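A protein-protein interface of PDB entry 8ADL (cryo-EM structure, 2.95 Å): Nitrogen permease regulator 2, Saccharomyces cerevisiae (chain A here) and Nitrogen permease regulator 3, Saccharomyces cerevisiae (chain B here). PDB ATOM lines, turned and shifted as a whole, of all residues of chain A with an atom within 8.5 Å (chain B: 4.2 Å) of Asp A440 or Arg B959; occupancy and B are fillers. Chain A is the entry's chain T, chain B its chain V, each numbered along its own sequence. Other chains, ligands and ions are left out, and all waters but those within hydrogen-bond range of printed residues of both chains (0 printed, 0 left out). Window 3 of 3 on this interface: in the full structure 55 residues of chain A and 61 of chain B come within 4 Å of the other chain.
Hydrophobic or aromatic side chains of chain A that line the printed part of chain B: Leu A325 and Phe A439. Printed residues of chain B that touch a printed residue of chain A: Asn B957, Arg B959, Tyr B1070, Ile B1072 and Ile B1141. Hydrophobic or aromatic side chains of chain B that line the printed part of chain A: Tyr B1070, Ile B1072 and Ile B1141. Among the printed residues, Asp or Glu carboxylates within 4 Å of a Lys or Arg side-chain nitrogen of the other chain: Asp A440 with Arg B959 (2.8 Å).
The backbone NH of Arg B959 sits at hydrogen-bond distance from the backbone carbonyl oxygen of Tyr B1139, 2.6 Å away. The backbone carbonyl oxygen (O) of Lys B1138 lies within hydrogen-bond range of the guanidinium group (NH2) of Arg B959 (3.0 Å). The backbone carbonyl oxygen (O) of Asn B957 sits at hydrogen-bond distance from the backbone NH (N) of Ile B1141 (2.5 Å). NH2 of Arg A443 is in salt-bridge range of OD1 of Asp A440 (3.1 Å).
Asp A440 touches two residues of chain B. No residue of chain A comes within 4 Å of Ile B958. Of the printed residues of chain A, Ile B1141 touches Phe A439 (3.6 Å), Asp A440 (3.9 Å) and Arg A443 (3.5 Å). Of the printed residues of chain A, Asn B957 touches Leu A325. Ile A461 touches none of the printed residues of chain B. Tyr B1139 touches none of the printed residues of chain A. The nearest residue of chain A that does not touch Arg B959 is Ser A436 (5.0 Å).
Among the printed residues, merely in contact across the chains: Leu A325 with Asn B957, Arg A443 with Ile B1141, Ser A436 with Tyr B1070, Phe A439 with Ile B1141, Leu A325 with Ile B1072, Asp A440 with Ile B1141 and Arg A443 with Arg B959.
The guanidinium group (NH1) of Arg B959 lies within salt-bridge range of the side-chain carboxylate (OD2) of Asp A440 (2.8 Å).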
ATOM      1  N   ILE A 321       7.630  -0.388  15.339  1.00  0.00           N
ATOM      2  CA  ILE A 321       7.499   0.209  16.662  1.00  0.00           C
ATOM      3  C   ILE A 321       8.711   1.077  16.991  1.00  0.00           C
ATOM      4  O   ILE A 321       8.601   2.028  17.775  1.00  0.00           O
ATOM      5  CB  ILE A 321       7.262  -0.910  17.703  1.00  0.00           C
ATOM      6  CG1 ILE A 321       6.944  -0.341  19.089  1.00  0.00           C
ATOM      7  CG2 ILE A 321       8.448  -1.864  17.763  1.00  0.00           C
ATOM      8  CD1 ILE A 321       5.580   0.302  19.182  1.00  0.00           C
ATOM      9  N   PHE A 324       8.560   4.963  16.534  1.00  0.00           N
ATOM     10  CA  PHE A 324       8.226   5.828  17.657  1.00  0.00           C
ATOM     11  C   PHE A 324       9.477   6.433  18.273  1.00  0.00           C
ATOM     12  O   PHE A 324       9.405   7.498  18.894  1.00  0.00           O
ATOM     13  CB  PHE A 324       7.440   5.048  18.712  1.00  0.00           C
ATOM     14  CG  PHE A 324       6.597   5.913  19.605  1.00  0.00           C
ATOM     15  CD1 PHE A 324       5.338   6.330  19.199  1.00  0.00           C
ATOM     16  CD2 PHE A 324       7.060   6.305  20.850  1.00  0.00           C
ATOM     17  CE1 PHE A 324       4.558   7.125  20.018  1.00  0.00           C
ATOM     18  CE2 PHE A 324       6.285   7.102  21.676  1.00  0.00           C
ATOM     19  CZ  PHE A 324       5.032   7.511  21.259  1.00  0.00           C
ATOM     20  N   LEU A 325      10.618   5.766  18.109  1.00  0.00           N
ATOM     21  CA  LEU A 325      11.912   6.216  18.596  1.00  0.00           C
ATOM     22  C   LEU A 325      12.664   7.005  17.536  1.00  0.00           C
ATOM     23  O   LEU A 325      13.232   8.061  17.834  1.00  0.00           O
ATOM     24  CB  LEU A 325      12.756   5.018  19.035  1.00  0.00           C
ATOM     25  CG  LEU A 325      12.236   4.217  20.224  1.00  0.00           C
ATOM     26  CD1 LEU A 325      13.080   2.971  20.441  1.00  0.00           C
ATOM     27  CD2 LEU A 325      12.224   5.087  21.454  1.00  0.00           C
ATOM     28  N   THR A 434       5.063  11.420  29.701  1.00  0.00           N
ATOM     29  CA  THR A 434       6.347  11.380  29.022  1.00  0.00           C
ATOM     30  C   THR A 434       6.336  10.342  27.900  1.00  0.00           C
ATOM     31  O   THR A 434       5.539   9.399  27.891  1.00  0.00           O
ATOM     32  CB  THR A 434       7.478  11.080  30.008  1.00  0.00           C
ATOM     33  OG1 THR A 434       8.719  10.980  29.299  1.00  0.00           O
ATOM     34  CG2 THR A 434       7.216   9.780  30.752  1.00  0.00           C
ATOM     35  N   ARG A 435       7.234  10.546  26.935  1.00  0.00           N
ATOM     36  CA  ARG A 435       7.298   9.681  25.762  1.00  0.00           C
ATOM     37  C   ARG A 435       7.782   8.277  26.108  1.00  0.00           C
ATOM     38  O   ARG A 435       7.423   7.312  25.419  1.00  0.00           O
ATOM     39  CB  ARG A 435       8.210  10.319  24.716  1.00  0.00           C
ATOM     40  CG  ARG A 435       7.965  11.811  24.534  1.00  0.00           C
ATOM     41  CD  ARG A 435       9.150  12.504  23.883  1.00  0.00           C
ATOM     42  NE  ARG A 435       8.837  13.872  23.489  1.00  0.00           N
ATOM     43  CZ  ARG A 435       9.542  14.936  23.849  1.00  0.00           C
ATOM     44  NH1 ARG A 435      10.616  14.826  24.615  1.00  0.00           N
ATOM     45  NH2 ARG A 435       9.161  16.139  23.431  1.00  0.00           N
ATOM     46  N   SER A 436       8.584   8.144  27.169  1.00  0.00           N
ATOM     47  CA  SER A 436       9.004   6.825  27.632  1.00  0.00           C
ATOM     48  C   SER A 436       7.816   6.019  28.139  1.00  0.00           C
ATOM     49  O   SER A 436       7.735   4.807  27.904  1.00  0.00           O
ATOM     50  CB  SER A 436      10.067   6.967  28.719  1.00  0.00           C
ATOM     51  OG  SER A 436      11.210   7.642  28.226  1.00  0.00           O
ATOM     52  N   CYS A 437       6.886   6.681  28.836  1.00  0.00           N
ATOM     53  CA  CYS A 437       5.663   6.024  29.290  1.00  0.00           C
ATOM     54  C   CYS A 437       4.824   5.542  28.114  1.00  0.00           C
ATOM     55  O   CYS A 437       4.283   4.428  28.142  1.00  0.00           O
ATOM     56  CB  CYS A 437       4.857   6.982  30.165  1.00  0.00           C
ATOM     57  SG  CYS A 437       3.284   6.322  30.739  1.00  0.00           S
ATOM     58  N   LEU A 438       4.709   6.368  27.069  1.00  0.00           N
ATOM     59  CA  LEU A 438       3.939   5.981  25.891  1.00  0.00           C
ATOM     60  C   LEU A 438       4.591   4.806  25.173  1.00  0.00           C
ATOM     61  O   LEU A 438       3.897   3.887  24.720  1.00  0.00           O
ATOM     62  CB  LEU A 438       3.790   7.171  24.946  1.00  0.00           C
ATOM     63  CG  LEU A 438       3.121   8.415  25.532  1.00  0.00           C
ATOM     64  CD1 LEU A 438       3.323   9.610  24.615  1.00  0.00           C
ATOM     65  CD2 LEU A 438       1.641   8.164  25.773  1.00  0.00           C
ATOM     66  N   PHE A 439       5.923   4.810  25.077  1.00  0.00           N
ATOM     67  CA  PHE A 439       6.621   3.692  24.451  1.00  0.00           C
ATOM     68  C   PHE A 439       6.458   2.410  25.265  1.00  0.00           C
ATOM     69  O   PHE A 439       6.257   1.331  24.696  1.00  0.00           O
ATOM     70  CB  PHE A 439       8.099   4.027  24.267  1.00  0.00           C
ATOM     71  CG  PHE A 439       8.832   3.053  23.393  1.00  0.00           C
ATOM     72  CD1 PHE A 439       8.449   2.866  22.074  1.00  0.00           C
ATOM     73  CD2 PHE A 439       9.896   2.320  23.889  1.00  0.00           C
ATOM     74  CE1 PHE A 439       9.118   1.969  21.262  1.00  0.00           C
ATOM     75  CE2 PHE A 439      10.571   1.422  23.084  1.00  0.00           C
ATOM     76  CZ  PHE A 439      10.180   1.244  21.769  1.00  0.00           C
ATOM     77  N   ASP A 440       6.531   2.514  26.597  1.00  0.00           N
ATOM     78  CA  ASP A 440       6.347   1.344  27.451  1.00  0.00           C
ATOM     79  C   ASP A 440       4.919   0.818  27.384  1.00  0.00           C
ATOM     80  O   ASP A 440       4.697  -0.390  27.534  1.00  0.00           O
ATOM     81  CB  ASP A 440       6.715   1.680  28.895  1.00  0.00           C
ATOM     82  CG  ASP A 440       8.199   1.924  29.075  1.00  0.00           C
ATOM     83  OD1 ASP A 440       8.920   1.982  28.058  1.00  0.00           O
ATOM     84  OD2 ASP A 440       8.643   2.056  30.234  1.00  0.00           O
ATOM     85  N   LEU A 441       3.944   1.701  27.161  1.00  0.00           N
ATOM     86  CA  LEU A 441       2.574   1.244  26.955  1.00  0.00           C
ATOM     87  C   LEU A 441       2.406   0.602  25.583  1.00  0.00           C
ATOM     88  O   LEU A 441       1.601  -0.324  25.428  1.00  0.00           O
ATOM     89  CB  LEU A 441       1.597   2.407  27.123  1.00  0.00           C
ATOM     90  CG  LEU A 441       1.333   2.865  28.558  1.00  0.00           C
ATOM     91  CD1 LEU A 441       0.444   4.097  28.573  1.00  0.00           C
ATOM     92  CD2 LEU A 441       0.715   1.741  29.376  1.00  0.00           C
ATOM     93  N   TYR A 442       3.153   1.076  24.584  1.00  0.00           N
ATOM     94  CA  TYR A 442       3.072   0.487  23.252  1.00  0.00           C
ATOM     95  C   TYR A 442       3.733  -0.885  23.197  1.00  0.00           C
ATOM     96  O   TYR A 442       3.287  -1.753  22.439  1.00  0.00           O
ATOM     97  CB  TYR A 442       3.710   1.421  22.222  1.00  0.00           C
ATOM     98  CG  TYR A 442       2.756   2.432  21.626  1.00  0.00           C
ATOM     99  CD1 TYR A 442       1.586   2.019  20.997  1.00  0.00           C
ATOM    100  CD2 TYR A 442       3.021   3.794  21.691  1.00  0.00           C
ATOM    101  CE1 TYR A 442       0.705   2.937  20.456  1.00  0.00           C
ATOM    102  CE2 TYR A 442       2.147   4.719  21.150  1.00  0.00           C
ATOM    103  CZ  TYR A 442       0.991   4.285  20.533  1.00  0.00           C
ATOM    104  OH  TYR A 442       0.119   5.201  19.991  1.00  0.00           O
ATOM    105  N   ARG A 443       4.794  -1.098  23.981  1.00  0.00           N
ATOM    106  CA  ARG A 443       5.439  -2.409  24.009  1.00  0.00           C
ATOM    107  C   ARG A 443       4.572  -3.458  24.698  1.00  0.00           C
ATOM    108  O   ARG A 443       4.570  -4.626  24.293  1.00  0.00           O
ATOM    109  CB  ARG A 443       6.798  -2.323  24.700  1.00  0.00           C
ATOM    110  CG  ARG A 443       7.801  -1.421  24.017  1.00  0.00           C
ATOM    111  CD  ARG A 443       9.126  -1.441  24.751  1.00  0.00           C
ATOM    112  NE  ARG A 443       9.010  -0.949  26.117  1.00  0.00           N
ATOM    113  CZ  ARG A 443       9.212  -1.691  27.199  1.00  0.00           C
ATOM    114  NH1 ARG A 443       9.544  -2.969  27.108  1.00  0.00           N
ATOM    115  NH2 ARG A 443       9.077  -1.137  28.400  1.00  0.00           N
ATOM    116  N   SER A 444       3.841  -3.065  25.745  1.00  0.00           N
ATOM    117  CA  SER A 444       3.152  -4.017  26.613  1.00  0.00           C
ATOM    118  C   SER A 444       1.989  -4.742  25.943  1.00  0.00           C
ATOM    119  O   SER A 444       1.489  -5.718  26.512  1.00  0.00           O
ATOM    120  CB  SER A 444       2.655  -3.300  27.868  1.00  0.00           C
ATOM    121  OG  SER A 444       1.676  -2.328  27.545  1.00  0.00           O
ATOM    122  N   LEU A 445       1.539  -4.292  24.774  1.00  0.00           N
ATOM    123  CA  LEU A 445       0.581  -5.057  23.989  1.00  0.00           C
ATOM    124  C   LEU A 445       1.209  -6.359  23.499  1.00  0.00           C
ATOM    125  O   LEU A 445       2.422  -6.450  23.296  1.00  0.00           O
ATOM    126  CB  LEU A 445       0.078  -4.231  22.804  1.00  0.00           C
ATOM    127  CG  LEU A 445      -0.611  -2.914  23.164  1.00  0.00           C
ATOM    128  CD1 LEU A 445      -0.575  -1.946  21.992  1.00  0.00           C
ATOM    129  CD2 LEU A 445      -2.043  -3.163  23.611  1.00  0.00           C
ATOM    130  N   TRP A 454      -5.241  -6.125  28.952  1.00  0.00           N
ATOM    131  CA  TRP A 454      -4.138  -5.169  28.920  1.00  0.00           C
ATOM    132  C   TRP A 454      -4.493  -3.887  29.663  1.00  0.00           C
ATOM    133  O   TRP A 454      -3.647  -3.303  30.350  1.00  0.00           O
ATOM    134  CB  TRP A 454      -3.758  -4.860  27.471  1.00  0.00           C
ATOM    135  CG  TRP A 454      -2.666  -3.842  27.336  1.00  0.00           C
ATOM    136  CD1 TRP A 454      -1.323  -4.082  27.320  1.00  0.00           C
ATOM    137  CD2 TRP A 454      -2.820  -2.423  27.193  1.00  0.00           C
ATOM    138  NE1 TRP A 454      -0.633  -2.904  27.179  1.00  0.00           N
ATOM    139  CE2 TRP A 454      -1.528  -1.870  27.100  1.00  0.00           C
ATOM    140  CE3 TRP A 454      -3.925  -1.567  27.140  1.00  0.00           C
ATOM    141  CZ2 TRP A 454      -1.309  -0.502  26.954  1.00  0.00           C
ATOM    142  CZ3 TRP A 454      -3.705  -0.209  26.994  1.00  0.00           C
ATOM    143  CH2 TRP A 454      -2.409   0.310  26.903  1.00  0.00           C
ATOM    144  N   LYS A 458      -2.841  -2.522  33.241  1.00  0.00           N
ATOM    145  CA  LYS A 458      -2.223  -1.196  33.279  1.00  0.00           C
ATOM    146  C   LYS A 458      -3.349  -0.168  33.218  1.00  0.00           C
ATOM    147  O   LYS A 458      -3.699   0.322  32.143  1.00  0.00           O
ATOM    148  CB  LYS A 458      -1.218  -1.013  32.145  1.00  0.00           C
ATOM    149  CG  LYS A 458       0.019  -1.886  32.278  1.00  0.00           C
ATOM    150  CD  LYS A 458       1.010  -1.631  31.157  1.00  0.00           C
ATOM    151  CE  LYS A 458       2.324  -2.346  31.422  1.00  0.00           C
ATOM    152  NZ  LYS A 458       2.169  -3.827  31.380  1.00  0.00           N
ATOM    153  N   ILE A 461      -1.548   3.575  35.429  1.00  0.00           N
ATOM    154  CA  ILE A 461      -0.673   4.392  34.591  1.00  0.00           C
ATOM    155  C   ILE A 461      -1.490   5.343  33.724  1.00  0.00           C
ATOM    156  O   ILE A 461      -1.200   6.545  33.651  1.00  0.00           O
ATOM    157  CB  ILE A 461       0.232   3.482  33.742  1.00  0.00           C
ATOM    158  CG1 ILE A 461       1.092   2.594  34.644  1.00  0.00           C
ATOM    159  CG2 ILE A 461       1.106   4.306  32.823  1.00  0.00           C
ATOM    160  CD1 ILE A 461       1.932   1.587  33.890  1.00  0.00           C
ATOM    161  N   PHE A 472      -5.049   6.415  22.031  1.00  0.00           N
ATOM    162  CA  PHE A 472      -3.759   5.730  22.022  1.00  0.00           C
ATOM    163  C   PHE A 472      -3.719   4.640  20.953  1.00  0.00           C
ATOM    164  O   PHE A 472      -2.763   4.556  20.168  1.00  0.00           O
ATOM    165  CB  PHE A 472      -3.515   5.167  23.427  1.00  0.00           C
ATOM    166  CG  PHE A 472      -2.360   4.216  23.541  1.00  0.00           C
ATOM    167  CD1 PHE A 472      -1.066   4.689  23.697  1.00  0.00           C
ATOM    168  CD2 PHE A 472      -2.578   2.846  23.576  1.00  0.00           C
ATOM    169  CE1 PHE A 472      -0.008   3.811  23.834  1.00  0.00           C
ATOM    170  CE2 PHE A 472      -1.526   1.964  23.710  1.00  0.00           C
ATOM    171  CZ  PHE A 472      -0.241   2.448  23.845  1.00  0.00           C
ATOM    172  N   ASN B 957      16.737  -2.866  23.025  1.00  0.00           N
ATOM    173  CA  ASN B 957      17.254  -1.506  23.007  1.00  0.00           C
ATOM    174  C   ASN B 957      17.628  -1.119  24.432  1.00  0.00           C
ATOM    175  O   ASN B 957      17.083  -1.662  25.397  1.00  0.00           O
ATOM    176  CB  ASN B 957      16.237  -0.514  22.430  1.00  0.00           C
ATOM    177  CG  ASN B 957      16.896   0.598  21.638  1.00  0.00           C
ATOM    178  OD1 ASN B 957      18.113   0.774  21.689  1.00  0.00           O
ATOM    179  ND2 ASN B 957      16.094   1.358  20.904  1.00  0.00           N
ATOM    180  N   ILE B 958      18.569  -0.187  24.566  1.00  0.00           N
ATOM    181  CA  ILE B 958      19.157   0.151  25.859  1.00  0.00           C
ATOM    182  C   ILE B 958      18.602   1.492  26.329  1.00  0.00           C
ATOM    183  O   ILE B 958      18.459   2.436  25.540  1.00  0.00           O
ATOM    184  CB  ILE B 958      20.701   0.153  25.786  1.00  0.00           C
ATOM    185  CG1 ILE B 958      21.323   0.495  27.145  1.00  0.00           C
ATOM    186  CG2 ILE B 958      21.220   1.059  24.666  1.00  0.00           C
ATOM    187  CD1 ILE B 958      21.170  -0.599  28.179  1.00  0.00           C
ATOM    188  N   ARG B 959      18.247   1.557  27.613  1.00  0.00           N
ATOM    189  CA  ARG B 959      17.559   2.698  28.199  1.00  0.00           C
ATOM    190  C   ARG B 959      18.261   3.106  29.487  1.00  0.00           C
ATOM    191  O   ARG B 959      18.710   2.248  30.253  1.00  0.00           O
ATOM    192  CB  ARG B 959      16.093   2.356  28.485  1.00  0.00           C
ATOM    193  CG  ARG B 959      15.227   3.539  28.851  1.00  0.00           C
ATOM    194  CD  ARG B 959      13.774   3.126  28.975  1.00  0.00           C
ATOM    195  NE  ARG B 959      13.609   2.107  30.006  1.00  0.00           N
ATOM    196  CZ  ARG B 959      12.458   1.527  30.310  1.00  0.00           C
ATOM    197  NH1 ARG B 959      11.336   1.857  29.693  1.00  0.00           N
ATOM    198  NH2 ARG B 959      12.430   0.602  31.264  1.00  0.00           N
ATOM    199  N   VAL B 960      18.357   4.414  29.728  1.00  0.00           N
ATOM    200  CA  VAL B 960      19.102   4.954  30.860  1.00  0.00           C
ATOM    201  C   VAL B 960      18.192   5.895  31.643  1.00  0.00           C
ATOM    202  O   VAL B 960      17.585   6.802  31.061  1.00  0.00           O
ATOM    203  CB  VAL B 960      20.380   5.681  30.394  1.00  0.00           C
ATOM    204  CG1 VAL B 960      20.919   6.607  31.476  1.00  0.00           C
ATOM    205  CG2 VAL B 960      21.440   4.675  29.981  1.00  0.00           C
ATOM    206  N   TYR B1070      14.000   9.588  32.085  1.00  0.00           N
ATOM    207  CA  TYR B1070      14.567   8.480  31.339  1.00  0.00           C
ATOM    208  C   TYR B1070      15.221   8.988  30.057  1.00  0.00           C
ATOM    209  O   TYR B1070      15.125  10.165  29.702  1.00  0.00           O
ATOM    210  CB  TYR B1070      13.481   7.466  30.986  1.00  0.00           C
ATOM    211  CG  TYR B1070      13.328   6.314  31.950  1.00  0.00           C
ATOM    212  CD1 TYR B1070      14.094   5.168  31.823  1.00  0.00           C
ATOM    213  CD2 TYR B1070      12.361   6.345  32.942  1.00  0.00           C
ATOM    214  CE1 TYR B1070      13.940   4.102  32.689  1.00  0.00           C
ATOM    215  CE2 TYR B1070      12.195   5.285  33.813  1.00  0.00           C
ATOM    216  CZ  TYR B1070      12.988   4.167  33.682  1.00  0.00           C
ATOM    217  OH  TYR B1070      12.826   3.110  34.547  1.00  0.00           O
ATOM    218  N   THR B1071      15.875   8.073  29.340  1.00  0.00           N
ATOM    219  CA  THR B1071      16.538   8.351  28.071  1.00  0.00           C
ATOM    220  C   THR B1071      16.833   7.019  27.394  1.00  0.00           C
ATOM    221  O   THR B1071      17.314   6.086  28.041  1.00  0.00           O
ATOM    222  CB  THR B1071      17.841   9.154  28.271  1.00  0.00           C
ATOM    223  OG1 THR B1071      17.526  10.475  28.730  1.00  0.00           O
ATOM    224  CG2 THR B1071      18.651   9.268  26.983  1.00  0.00           C
ATOM    225  N   ILE B1072      16.545   6.939  26.098  1.00  0.00           N
ATOM    226  CA  ILE B1072      16.793   5.743  25.303  1.00  0.00           C
ATOM    227  C   ILE B1072      17.965   6.032  24.374  1.00  0.00           C
ATOM    228  O   ILE B1072      17.869   6.894  23.490  1.00  0.00           O
ATOM    229  CB  ILE B1072      15.544   5.302  24.531  1.00  0.00           C
ATOM    230  CG1 ILE B1072      14.459   4.883  25.527  1.00  0.00           C
ATOM    231  CG2 ILE B1072      15.878   4.162  23.582  1.00  0.00           C
ATOM    232  CD1 ILE B1072      13.192   4.364  24.908  1.00  0.00           C
ATOM    233  N   LYS B1138      15.152  -2.992  34.036  1.00  0.00           N
ATOM    234  CA  LYS B1138      14.742  -1.610  33.818  1.00  0.00           C
ATOM    235  C   LYS B1138      15.585  -0.881  32.781  1.00  0.00           C
ATOM    236  O   LYS B1138      15.178   0.192  32.325  1.00  0.00           O
ATOM    237  CB  LYS B1138      14.788  -0.840  35.140  1.00  0.00           C
ATOM    238  CG  LYS B1138      15.988  -1.179  36.011  1.00  0.00           C
ATOM    239  CD  LYS B1138      15.839  -0.602  37.408  1.00  0.00           C
ATOM    240  CE  LYS B1138      17.032  -0.957  38.282  1.00  0.00           C
ATOM    241  NZ  LYS B1138      17.207  -2.430  38.410  1.00  0.00           N
ATOM    242  N   TYR B1139      16.737  -1.429  32.394  1.00  0.00           N
ATOM    243  CA  TYR B1139      17.622  -0.753  31.456  1.00  0.00           C
ATOM    244  C   TYR B1139      17.482  -1.257  30.028  1.00  0.00           C
ATOM    245  O   TYR B1139      17.896  -0.558  29.097  1.00  0.00           O
ATOM    246  CB  TYR B1139      19.081  -0.900  31.900  1.00  0.00           C
ATOM    247  CG  TYR B1139      19.350  -0.361  33.286  1.00  0.00           C
ATOM    248  CD1 TYR B1139      19.166   0.984  33.574  1.00  0.00           C
ATOM    249  CD2 TYR B1139      19.786  -1.198  34.305  1.00  0.00           C
ATOM    250  CE1 TYR B1139      19.410   1.482  34.841  1.00  0.00           C
ATOM    251  CE2 TYR B1139      20.033  -0.710  35.575  1.00  0.00           C
ATOM    252  CZ  TYR B1139      19.843   0.631  35.836  1.00  0.00           C
ATOM    253  OH  TYR B1139      20.086   1.123  37.098  1.00  0.00           O
ATOM    254  N   ILE B1141      15.157  -2.363  26.854  1.00  0.00           N
ATOM    255  CA  ILE B1141      13.854  -2.275  26.211  1.00  0.00           C
ATOM    256  C   ILE B1141      13.602  -3.589  25.486  1.00  0.00           C
ATOM    257  O   ILE B1141      14.453  -4.061  24.722  1.00  0.00           O
ATOM    258  CB  ILE B1141      13.806  -1.076  25.246  1.00  0.00           C
ATOM    259  CG1 ILE B1141      13.586   0.224  26.024  1.00  0.00           C
ATOM    260  CG2 ILE B1141      12.750  -1.262  24.167  1.00  0.00           C
ATOM    261  CD1 ILE B1141      12.218   0.331  26.661  1.00  0.00           C
